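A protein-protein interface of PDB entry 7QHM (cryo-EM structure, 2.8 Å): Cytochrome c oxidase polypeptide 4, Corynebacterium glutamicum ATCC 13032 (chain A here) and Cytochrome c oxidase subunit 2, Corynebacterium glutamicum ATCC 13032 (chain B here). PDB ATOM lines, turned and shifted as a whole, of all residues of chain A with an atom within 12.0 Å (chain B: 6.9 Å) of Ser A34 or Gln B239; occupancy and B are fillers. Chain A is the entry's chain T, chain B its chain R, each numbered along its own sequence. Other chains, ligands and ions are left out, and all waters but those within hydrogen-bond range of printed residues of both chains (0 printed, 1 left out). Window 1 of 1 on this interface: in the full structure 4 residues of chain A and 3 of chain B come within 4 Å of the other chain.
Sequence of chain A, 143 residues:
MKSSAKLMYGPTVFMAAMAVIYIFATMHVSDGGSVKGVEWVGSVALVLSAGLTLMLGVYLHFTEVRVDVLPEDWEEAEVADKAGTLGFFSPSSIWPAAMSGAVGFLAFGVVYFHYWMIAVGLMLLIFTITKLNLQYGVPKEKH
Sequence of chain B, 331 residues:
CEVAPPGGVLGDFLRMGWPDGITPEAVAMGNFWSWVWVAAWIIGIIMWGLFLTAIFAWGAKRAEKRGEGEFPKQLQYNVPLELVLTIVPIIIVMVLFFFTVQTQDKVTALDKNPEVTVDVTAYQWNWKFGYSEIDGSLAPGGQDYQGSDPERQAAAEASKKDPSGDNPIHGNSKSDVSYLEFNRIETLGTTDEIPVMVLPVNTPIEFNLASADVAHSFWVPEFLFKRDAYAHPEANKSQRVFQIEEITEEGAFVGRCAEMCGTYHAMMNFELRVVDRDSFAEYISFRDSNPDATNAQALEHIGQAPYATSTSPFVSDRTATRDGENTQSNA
The backbone carbonyl oxygen (O) of Gln B239 lies within hydrogen-bond range of the guanidinium group (NH1) of Arg B227, 3.0 Å away.
The backbone NH of Val B241 sits close to the side-chain amide oxygen of Gln B239, at 3.4 Å.
N of Ser A34 sits at hydrogen-bond distance from OD1 of Asp A31 (3.4 Å).
Among the printed residues, pairs that only touch across the chains: Gly A32 with Thr B108, Gly A32 with Gln B239, Gly A33 with Thr B108, Ser A34 with Gln B239, Val A35 with Lys B237 and Val A35 with Gln B239.
Of the printed residues of chain B, Ser A34 touches Gln B239 (3.998 Å).
Of the printed residues of chain A, Gln B239 touches Gly A32 (3.4 Å), Ser A34 (3.998 Å) and Val A35 (3.9 Å).
No residue of chain A comes within 4 Å of Ser B238.
Of the printed residues of chain A, Thr B108 touches Gly A32 and Gly A33.
Of the printed residues of chain A, Lys B237 touches Val A35.
Printed residues of chain B within 4 Å of Val A35: Lys B237 and Gln B239.
Of the printed residues of chain B, Gly A32 touches Thr B108 (3.3 Å) and Gln B239 (3.4 Å).
Tyr A22 touches none of the printed residues of chain B.
Thr A26 touches none of the printed residues of chain B.
The nearest printed residue of chain A that does not touch Gln B239 is Gly A33 (4.3 Å).
The nearest printed residue of chain B that does not touch Gly A32 is Leu B110 (4.02 Å).
Of the 15 printed residues of chain B, 3 touch a printed residue of chain A.
Among the printed residues, 6 pairs touch across the chains.
Among the printed residues, no Asp or Glu carboxylate lies within 4 Å of a Lys or Arg side-chain nitrogen of the other chain.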
ATOM      1  N   TYR A  22     -30.833  18.336 -21.865  1.00  0.00           N
ATOM      2  CA  TYR A  22     -29.551  18.632 -21.246  1.00  0.00           C
ATOM      3  C   TYR A  22     -29.359  20.123 -21.067  1.00  0.00           C
ATOM      4  O   TYR A  22     -28.854  20.571 -20.037  1.00  0.00           O
ATOM      5  CB  TYR A  22     -28.435  18.055 -22.114  1.00  0.00           C
ATOM      6  CG  TYR A  22     -27.044  18.267 -21.579  1.00  0.00           C
ATOM      7  CD1 TYR A  22     -26.559  17.491 -20.550  1.00  0.00           C
ATOM      8  CD2 TYR A  22     -26.212  19.225 -22.128  1.00  0.00           C
ATOM      9  CE1 TYR A  22     -25.290  17.673 -20.069  1.00  0.00           C
ATOM     10  CE2 TYR A  22     -24.943  19.415 -21.652  1.00  0.00           C
ATOM     11  CZ  TYR A  22     -24.484  18.637 -20.625  1.00  0.00           C
ATOM     12  OH  TYR A  22     -23.213  18.821 -20.146  1.00  0.00           O
ATOM     13  N   ILE A  23     -29.775  20.909 -22.051  1.00  0.00           N
ATOM     14  CA  ILE A  23     -29.554  22.346 -21.997  1.00  0.00           C
ATOM     15  C   ILE A  23     -30.341  22.959 -20.847  1.00  0.00           C
ATOM     16  O   ILE A  23     -29.772  23.605 -19.951  1.00  0.00           O
ATOM     17  CB  ILE A  23     -29.917  22.973 -23.352  1.00  0.00           C
ATOM     18  CG1 ILE A  23     -28.812  22.655 -24.360  1.00  0.00           C
ATOM     19  CG2 ILE A  23     -30.094  24.456 -23.246  1.00  0.00           C
ATOM     20  CD1 ILE A  23     -29.263  22.599 -25.799  1.00  0.00           C
ATOM     21  N   PHE A  24     -31.665  22.757 -20.854  1.00  0.00           N
ATOM     22  CA  PHE A  24     -32.493  23.310 -19.786  1.00  0.00           C
ATOM     23  C   PHE A  24     -32.053  22.799 -18.425  1.00  0.00           C
ATOM     24  O   PHE A  24     -32.009  23.560 -17.448  1.00  0.00           O
ATOM     25  CB  PHE A  24     -33.958  22.957 -20.007  1.00  0.00           C
ATOM     26  CG  PHE A  24     -34.658  23.819 -21.009  1.00  0.00           C
ATOM     27  CD1 PHE A  24     -34.842  25.165 -20.781  1.00  0.00           C
ATOM     28  CD2 PHE A  24     -35.174  23.268 -22.157  1.00  0.00           C
ATOM     29  CE1 PHE A  24     -35.496  25.943 -21.688  1.00  0.00           C
ATOM     30  CE2 PHE A  24     -35.830  24.039 -23.066  1.00  0.00           C
ATOM     31  CZ  PHE A  24     -35.994  25.382 -22.834  1.00  0.00           C
ATOM     32  N   ALA A  25     -31.711  21.515 -18.341  1.00  0.00           N
ATOM     33  CA  ALA A  25     -31.360  20.930 -17.062  1.00  0.00           C
ATOM     34  C   ALA A  25     -30.072  21.528 -16.525  1.00  0.00           C
ATOM     35  O   ALA A  25     -29.991  21.891 -15.346  1.00  0.00           O
ATOM     36  CB  ALA A  25     -31.231  19.419 -17.207  1.00  0.00           C
ATOM     37  N   THR A  26     -29.046  21.640 -17.368  1.00  0.00           N
ATOM     38  CA  THR A  26     -27.780  22.142 -16.865  1.00  0.00           C
ATOM     39  C   THR A  26     -27.870  23.610 -16.509  1.00  0.00           C
ATOM     40  O   THR A  26     -27.104  24.071 -15.659  1.00  0.00           O
ATOM     41  CB  THR A  26     -26.651  21.921 -17.870  1.00  0.00           C
ATOM     42  OG1 THR A  26     -27.008  22.470 -19.141  1.00  0.00           O
ATOM     43  CG2 THR A  26     -26.337  20.440 -18.002  1.00  0.00           C
ATOM     44  N   MET A  27     -28.793  24.364 -17.120  1.00  0.00           N
ATOM     45  CA  MET A  27     -28.886  25.771 -16.735  1.00  0.00           C
ATOM     46  C   MET A  27     -29.789  26.024 -15.535  1.00  0.00           C
ATOM     47  O   MET A  27     -29.529  26.973 -14.788  1.00  0.00           O
ATOM     48  CB  MET A  27     -29.343  26.633 -17.907  1.00  0.00           C
ATOM     49  CG  MET A  27     -30.783  26.521 -18.319  1.00  0.00           C
ATOM     50  SD  MET A  27     -31.104  27.619 -19.705  1.00  0.00           S
ATOM     51  CE  MET A  27     -30.094  26.851 -20.960  1.00  0.00           C
ATOM     52  N   HIS A  28     -30.822  25.210 -15.318  1.00  0.00           N
ATOM     53  CA  HIS A  28     -31.772  25.454 -14.237  1.00  0.00           C
ATOM     54  C   HIS A  28     -31.556  24.574 -13.010  1.00  0.00           C
ATOM     55  O   HIS A  28     -31.618  25.075 -11.887  1.00  0.00           O
ATOM     56  CB  HIS A  28     -33.201  25.264 -14.740  1.00  0.00           C
ATOM     57  CG  HIS A  28     -34.236  25.507 -13.691  1.00  0.00           C
ATOM     58  ND1 HIS A  28     -34.408  26.734 -13.088  1.00  0.00           N
ATOM     59  CD2 HIS A  28     -35.147  24.680 -13.126  1.00  0.00           C
ATOM     60  CE1 HIS A  28     -35.385  26.654 -12.203  1.00  0.00           C
ATOM     61  NE2 HIS A  28     -35.849  25.418 -12.205  1.00  0.00           N
ATOM     62  N   VAL A  29     -31.307  23.275 -13.180  1.00  0.00           N
ATOM     63  CA  VAL A  29     -31.217  22.382 -12.027  1.00  0.00           C
ATOM     64  C   VAL A  29     -29.950  22.674 -11.229  1.00  0.00           C
ATOM     65  O   VAL A  29     -28.915  23.071 -11.778  1.00  0.00           O
ATOM     66  CB  VAL A  29     -31.262  20.907 -12.475  1.00  0.00           C
ATOM     67  CG1 VAL A  29     -31.183  19.965 -11.280  1.00  0.00           C
ATOM     68  CG2 VAL A  29     -32.523  20.633 -13.274  1.00  0.00           C
ATOM     69  N   SER A  30     -30.036  22.471  -9.913  1.00  0.00           N
ATOM     70  CA  SER A  30     -28.912  22.614  -8.998  1.00  0.00           C
ATOM     71  C   SER A  30     -28.789  21.367  -8.138  1.00  0.00           C
ATOM     72  O   SER A  30     -29.785  20.897  -7.579  1.00  0.00           O
ATOM     73  CB  SER A  30     -29.081  23.833  -8.096  1.00  0.00           C
ATOM     74  OG  SER A  30     -28.071  23.860  -7.105  1.00  0.00           O
ATOM     75  N   ASP A  31     -27.573  20.834  -8.041  1.00  0.00           N
ATOM     76  CA  ASP A  31     -27.246  19.809  -7.062  1.00  0.00           C
ATOM     77  C   ASP A  31     -25.901  20.156  -6.440  1.00  0.00           C
ATOM     78  O   ASP A  31     -25.119  20.925  -6.999  1.00  0.00           O
ATOM     79  CB  ASP A  31     -27.224  18.395  -7.678  1.00  0.00           C
ATOM     80  CG  ASP A  31     -26.231  18.252  -8.830  1.00  0.00           C
ATOM     81  OD1 ASP A  31     -25.464  19.197  -9.106  1.00  0.00           O
ATOM     82  OD2 ASP A  31     -26.227  17.178  -9.471  1.00  0.00           O
ATOM     83  N   GLY A  32     -25.627  19.565  -5.284  1.00  0.00           N
ATOM     84  CA  GLY A  32     -24.420  19.905  -4.560  1.00  0.00           C
ATOM     85  C   GLY A  32     -23.125  19.437  -5.187  1.00  0.00           C
ATOM     86  O   GLY A  32     -22.063  19.718  -4.628  1.00  0.00           O
ATOM     87  N   GLY A  33     -23.181  18.718  -6.310  1.00  0.00           N
ATOM     88  CA  GLY A  33     -22.004  18.168  -6.950  1.00  0.00           C
ATOM     89  C   GLY A  33     -21.722  18.783  -8.301  1.00  0.00           C
ATOM     90  O   GLY A  33     -21.067  18.163  -9.141  1.00  0.00           O
ATOM     91  N   SER A  34     -22.203  20.001  -8.526  1.00  0.00           N
ATOM     92  CA  SER A  34     -21.935  20.716  -9.761  1.00  0.00           C
ATOM     93  C   SER A  34     -22.423  22.145  -9.590  1.00  0.00           C
ATOM     94  O   SER A  34     -23.236  22.439  -8.713  1.00  0.00           O
ATOM     95  CB  SER A  34     -22.608  20.050 -10.963  1.00  0.00           C
ATOM     96  OG  SER A  34     -24.005  19.945 -10.781  1.00  0.00           O
ATOM     97  N   VAL A  35     -21.912  23.027 -10.441  1.00  0.00           N
ATOM     98  CA  VAL A  35     -22.253  24.443 -10.428  1.00  0.00           C
ATOM     99  C   VAL A  35     -23.248  24.703 -11.545  1.00  0.00           C
ATOM    100  O   VAL A  35     -23.075  24.225 -12.671  1.00  0.00           O
ATOM    101  CB  VAL A  35     -20.996  25.320 -10.586  1.00  0.00           C
ATOM    102  CG1 VAL A  35     -21.352  26.791 -10.476  1.00  0.00           C
ATOM    103  CG2 VAL A  35     -19.948  24.952  -9.542  1.00  0.00           C
ATOM    104  N   LYS A  36     -24.290  25.467 -11.235  1.00  0.00           N
ATOM    105  CA  LYS A  36     -25.341  25.738 -12.203  1.00  0.00           C
ATOM    106  C   LYS A  36     -24.826  26.613 -13.333  1.00  0.00           C
ATOM    107  O   LYS A  36     -24.093  27.579 -13.109  1.00  0.00           O
ATOM    108  CB  LYS A  36     -26.512  26.424 -11.518  1.00  0.00           C
ATOM    109  CG  LYS A  36     -27.781  26.497 -12.343  1.00  0.00           C
ATOM    110  CD  LYS A  36     -28.826  27.387 -11.688  1.00  0.00           C
ATOM    111  CE  LYS A  36     -29.298  26.853 -10.345  1.00  0.00           C
ATOM    112  NZ  LYS A  36     -30.394  27.680  -9.775  1.00  0.00           N
ATOM    113  N   GLY A  37     -25.230  26.275 -14.552  1.00  0.00           N
ATOM    114  CA  GLY A  37     -24.872  27.027 -15.736  1.00  0.00           C
ATOM    115  C   GLY A  37     -24.970  26.147 -16.961  1.00  0.00           C
ATOM    116  O   GLY A  37     -24.751  24.939 -16.857  1.00  0.00           O
ATOM    117  N   VAL A  38     -25.296  26.717 -18.120  1.00  0.00           N
ATOM    118  CA  VAL A  38     -25.435  25.910 -19.325  1.00  0.00           C
ATOM    119  C   VAL A  38     -24.070  25.368 -19.726  1.00  0.00           C
ATOM    120  O   VAL A  38     -23.076  26.103 -19.765  1.00  0.00           O
ATOM    121  CB  VAL A  38     -26.093  26.725 -20.451  1.00  0.00           C
ATOM    122  CG1 VAL A  38     -25.120  27.689 -21.107  1.00  0.00           C
ATOM    123  CG2 VAL A  38     -26.694  25.808 -21.486  1.00  0.00           C
ATOM    124  N   GLU A  39     -24.010  24.068 -19.999  1.00  0.00           N
ATOM    125  CA  GLU A  39     -22.764  23.392 -20.345  1.00  0.00           C
ATOM    126  C   GLU A  39     -22.640  23.367 -21.863  1.00  0.00           C
ATOM    127  O   GLU A  39     -23.339  22.610 -22.540  1.00  0.00           O
ATOM    128  CB  GLU A  39     -22.743  21.986 -19.754  1.00  0.00           C
ATOM    129  CG  GLU A  39     -21.356  21.392 -19.591  1.00  0.00           C
ATOM    130  CD  GLU A  39     -20.759  20.927 -20.898  1.00  0.00           C
ATOM    131  OE1 GLU A  39     -21.156  19.845 -21.378  1.00  0.00           O
ATOM    132  OE2 GLU A  39     -19.905  21.647 -21.453  1.00  0.00           O
ATOM    133  N   THR B 108     -24.035  14.220  -1.347  1.00  0.00           N
ATOM    134  CA  THR B 108     -23.593  15.391  -2.087  1.00  0.00           C
ATOM    135  C   THR B 108     -24.160  16.701  -1.541  1.00  0.00           C
ATOM    136  O   THR B 108     -23.811  17.770  -2.043  1.00  0.00           O
ATOM    137  CB  THR B 108     -23.968  15.187  -3.564  1.00  0.00           C
ATOM    138  OG1 THR B 108     -23.425  13.942  -4.020  1.00  0.00           O
ATOM    139  CG2 THR B 108     -23.433  16.265  -4.438  1.00  0.00           C
ATOM    140  N   LEU B 110     -24.822  20.112   0.582  1.00  0.00           N
ATOM    141  CA  LEU B 110     -24.013  21.139   1.230  1.00  0.00           C
ATOM    142  C   LEU B 110     -24.838  21.929   2.236  1.00  0.00           C
ATOM    143  O   LEU B 110     -24.914  23.157   2.157  1.00  0.00           O
ATOM    144  CB  LEU B 110     -23.417  22.095   0.195  1.00  0.00           C
ATOM    145  CG  LEU B 110     -22.389  21.538  -0.774  1.00  0.00           C
ATOM    146  CD1 LEU B 110     -22.076  22.585  -1.809  1.00  0.00           C
ATOM    147  CD2 LEU B 110     -21.128  21.118  -0.054  1.00  0.00           C
ATOM    148  N   ASN B 208     -12.304  22.118   1.399  1.00  0.00           N
ATOM    149  CA  ASN B 208     -12.325  23.085   0.305  1.00  0.00           C
ATOM    150  C   ASN B 208     -11.077  22.859  -0.539  1.00  0.00           C
ATOM    151  O   ASN B 208      -9.973  23.218  -0.126  1.00  0.00           O
ATOM    152  CB  ASN B 208     -12.381  24.508   0.855  1.00  0.00           C
ATOM    153  CG  ASN B 208     -12.456  25.551  -0.225  1.00  0.00           C
ATOM    154  OD1 ASN B 208     -13.124  25.366  -1.233  1.00  0.00           O
ATOM    155  ND2 ASN B 208     -11.765  26.660  -0.021  1.00  0.00           N
ATOM    156  N   LEU B 209     -11.253  22.283  -1.719  1.00  0.00           N
ATOM    157  CA  LEU B 209     -10.155  21.761  -2.517  1.00  0.00           C
ATOM    158  C   LEU B 209      -9.792  22.704  -3.653  1.00  0.00           C
ATOM    159  O   LEU B 209     -10.629  23.447  -4.161  1.00  0.00           O
ATOM    160  CB  LEU B 209     -10.525  20.404  -3.102  1.00  0.00           C
ATOM    161  CG  LEU B 209     -11.259  19.420  -2.196  1.00  0.00           C
ATOM    162  CD1 LEU B 209     -11.586  18.190  -2.989  1.00  0.00           C
ATOM    163  CD2 LEU B 209     -10.430  19.065  -0.998  1.00  0.00           C
ATOM    164  N   ARG B 227     -12.908  13.419  -4.623  1.00  0.00           N
ATOM    165  CA  ARG B 227     -13.235  14.491  -5.549  1.00  0.00           C
ATOM    166  C   ARG B 227     -11.962  15.043  -6.164  1.00  0.00           C
ATOM    167  O   ARG B 227     -10.908  15.064  -5.530  1.00  0.00           O
ATOM    168  CB  ARG B 227     -14.004  15.629  -4.876  1.00  0.00           C
ATOM    169  CG  ARG B 227     -14.414  16.703  -5.863  1.00  0.00           C
ATOM    170  CD  ARG B 227     -15.467  17.604  -5.332  1.00  0.00           C
ATOM    171  NE  ARG B 227     -16.736  16.918  -5.172  1.00  0.00           N
ATOM    172  CZ  ARG B 227     -17.833  17.477  -4.690  1.00  0.00           C
ATOM    173  NH1 ARG B 227     -17.861  18.746  -4.323  1.00  0.00           N
ATOM    174  NH2 ARG B 227     -18.932  16.745  -4.569  1.00  0.00           N
ATOM    175  N   ASP B 228     -12.075  15.486  -7.411  1.00  0.00           N
ATOM    176  CA  ASP B 228     -10.958  16.090  -8.114  1.00  0.00           C
ATOM    177  C   ASP B 228     -10.744  17.513  -7.637  1.00  0.00           C
ATOM    178  O   ASP B 228     -11.692  18.285  -7.500  1.00  0.00           O
ATOM    179  CB  ASP B 228     -11.203  16.112  -9.623  1.00  0.00           C
ATOM    180  CG  ASP B 228     -11.221  14.737 -10.244  1.00  0.00           C
ATOM    181  OD1 ASP B 228     -11.100  13.731  -9.519  1.00  0.00           O
ATOM    182  OD2 ASP B 228     -11.358  14.663 -11.477  1.00  0.00           O
ATOM    183  N   TYR B 230      -9.026  20.962  -8.746  1.00  0.00           N
ATOM    184  CA  TYR B 230      -8.668  21.619  -9.991  1.00  0.00           C
ATOM    185  C   TYR B 230      -8.033  22.972  -9.730  1.00  0.00           C
ATOM    186  O   TYR B 230      -8.234  23.584  -8.684  1.00  0.00           O
ATOM    187  CB  TYR B 230      -9.894  21.818 -10.878  1.00  0.00           C
ATOM    188  CG  TYR B 230     -10.436  20.540 -11.439  1.00  0.00           C
ATOM    189  CD1 TYR B 230      -9.775  19.881 -12.451  1.00  0.00           C
ATOM    190  CD2 TYR B 230     -11.603  19.996 -10.959  1.00  0.00           C
ATOM    191  CE1 TYR B 230     -10.257  18.723 -12.965  1.00  0.00           C
ATOM    192  CE2 TYR B 230     -12.095  18.838 -11.468  1.00  0.00           C
ATOM    193  CZ  TYR B 230     -11.417  18.201 -12.472  1.00  0.00           C
ATOM    194  OH  TYR B 230     -11.902  17.033 -12.994  1.00  0.00           O
ATOM    195  N   PRO B 233     -11.020  26.340  -9.835  1.00  0.00           N
ATOM    196  CA  PRO B 233     -12.226  25.496  -9.848  1.00  0.00           C
ATOM    197  C   PRO B 233     -13.473  26.207 -10.335  1.00  0.00           C
ATOM    198  O   PRO B 233     -14.382  25.551 -10.853  1.00  0.00           O
ATOM    199  CB  PRO B 233     -12.366  25.072  -8.381  1.00  0.00           C
ATOM    200  CG  PRO B 233     -11.041  25.275  -7.792  1.00  0.00           C
ATOM    201  CD  PRO B 233     -10.452  26.441  -8.482  1.00  0.00           C
ATOM    202  N   ASN B 236     -13.889  26.243 -14.170  1.00  0.00           N
ATOM    203  CA  ASN B 236     -14.295  24.924 -14.623  1.00  0.00           C
ATOM    204  C   ASN B 236     -15.677  24.525 -14.127  1.00  0.00           C
ATOM    205  O   ASN B 236     -16.154  23.444 -14.479  1.00  0.00           O
ATOM    206  CB  ASN B 236     -13.273  23.887 -14.161  1.00  0.00           C
ATOM    207  CG  ASN B 236     -11.934  24.029 -14.860  1.00  0.00           C
ATOM    208  OD1 ASN B 236     -11.703  23.421 -15.900  1.00  0.00           O
ATOM    209  ND2 ASN B 236     -11.043  24.822 -14.287  1.00  0.00           N
ATOM    210  N   LYS B 237     -16.333  25.366 -13.328  1.00  0.00           N
ATOM    211  CA  LYS B 237     -17.641  25.057 -12.749  1.00  0.00           C
ATOM    212  C   LYS B 237     -17.583  23.765 -11.937  1.00  0.00           C
ATOM    213  O   LYS B 237     -18.520  22.966 -11.928  1.00  0.00           O
ATOM    214  CB  LYS B 237     -18.730  24.995 -13.828  1.00  0.00           C
ATOM    215  CG  LYS B 237     -19.300  26.343 -14.238  1.00  0.00           C
ATOM    216  CD  LYS B 237     -18.399  27.127 -15.184  1.00  0.00           C
ATOM    217  CE  LYS B 237     -18.436  26.575 -16.597  1.00  0.00           C
ATOM    218  NZ  LYS B 237     -17.684  27.445 -17.539  1.00  0.00           N
ATOM    219  N   SER B 238     -16.474  23.566 -11.235  1.00  0.00           N
ATOM    220  CA  SER B 238     -16.258  22.385 -10.410  1.00  0.00           C
ATOM    221  C   SER B 238     -16.505  22.753  -8.957  1.00  0.00           C
ATOM    222  O   SER B 238     -15.782  23.581  -8.396  1.00  0.00           O
ATOM    223  CB  SER B 238     -14.844  21.844 -10.594  1.00  0.00           C
ATOM    224  OG  SER B 238     -14.545  20.880  -9.615  1.00  0.00           O
ATOM    225  N   GLN B 239     -17.528  22.149  -8.358  1.00  0.00           N
ATOM    226  CA  GLN B 239     -17.880  22.452  -6.981  1.00  0.00           C
ATOM    227  C   GLN B 239     -16.736  22.051  -6.075  1.00  0.00           C
ATOM    228  O   GLN B 239     -16.442  20.862  -5.931  1.00  0.00           O
ATOM    229  CB  GLN B 239     -19.169  21.734  -6.582  1.00  0.00           C
ATOM    230  CG  GLN B 239     -19.641  21.998  -5.155  1.00  0.00           C
ATOM    231  CD  GLN B 239     -19.715  23.473  -4.822  1.00  0.00           C
ATOM    232  OE1 GLN B 239     -18.745  24.063  -4.359  1.00  0.00           O
ATOM    233  NE2 GLN B 239     -20.861  24.082  -5.080  1.00  0.00           N
ATOM    234  N   ARG B 240     -16.086  23.036  -5.461  1.00  0.00           N
ATOM    235  CA  ARG B 240     -14.813  22.807  -4.797  1.00  0.00           C
ATOM    236  C   ARG B 240     -14.937  22.477  -3.319  1.00  0.00           C
ATOM    237  O   ARG B 240     -13.927  22.120  -2.709  1.00  0.00           O
ATOM    238  CB  ARG B 240     -13.901  24.026  -4.972  1.00  0.00           C
ATOM    239  CG  ARG B 240     -14.429  25.344  -4.427  1.00  0.00           C
ATOM    240  CD  ARG B 240     -13.470  26.470  -4.724  1.00  0.00           C
ATOM    241  NE  ARG B 240     -12.191  26.298  -4.048  1.00  0.00           N
ATOM    242  CZ  ARG B 240     -11.189  27.165  -4.091  1.00  0.00           C
ATOM    243  NH1 ARG B 240     -11.262  28.277  -4.800  1.00  0.00           N
ATOM    244  NH2 ARG B 240     -10.087  26.914  -3.395  1.00  0.00           N
ATOM    245  N   VAL B 241     -16.128  22.572  -2.728  1.00  0.00           N
ATOM    246  CA  VAL B 241     -16.337  22.262  -1.318  1.00  0.00           C
ATOM    247  C   VAL B 241     -17.178  21.001  -1.202  1.00  0.00           C
ATOM    248  O   VAL B 241     -18.088  20.772  -2.005  1.00  0.00           O
ATOM    249  CB  VAL B 241     -16.992  23.425  -0.542  1.00  0.00           C
ATOM    250  CG1 VAL B 241     -16.165  24.671  -0.672  1.00  0.00           C
ATOM    251  CG2 VAL B 241     -18.400  23.689  -0.998  1.00  0.00           C
ATOM    252  N   PHE B 242     -16.860  20.178  -0.204  1.00  0.00           N
ATOM    253  CA  PHE B 242     -17.742  19.094   0.196  1.00  0.00           C
ATOM    254  C   PHE B 242     -17.700  18.976   1.709  1.00  0.00           C
ATOM    255  O   PHE B 242     -16.772  19.447   2.362  1.00  0.00           O
ATOM    256  CB  PHE B 242     -17.394  17.771  -0.511  1.00  0.00           C
ATOM    257  CG  PHE B 242     -16.248  17.009   0.090  1.00  0.00           C
ATOM    258  CD1 PHE B 242     -14.950  17.241  -0.329  1.00  0.00           C
ATOM    259  CD2 PHE B 242     -16.474  16.013   1.026  1.00  0.00           C
ATOM    260  CE1 PHE B 242     -13.907  16.525   0.199  1.00  0.00           C
ATOM    261  CE2 PHE B 242     -15.436  15.303   1.561  1.00  0.00           C
ATOM    262  CZ  PHE B 242     -14.148  15.557   1.145  1.00  0.00           C
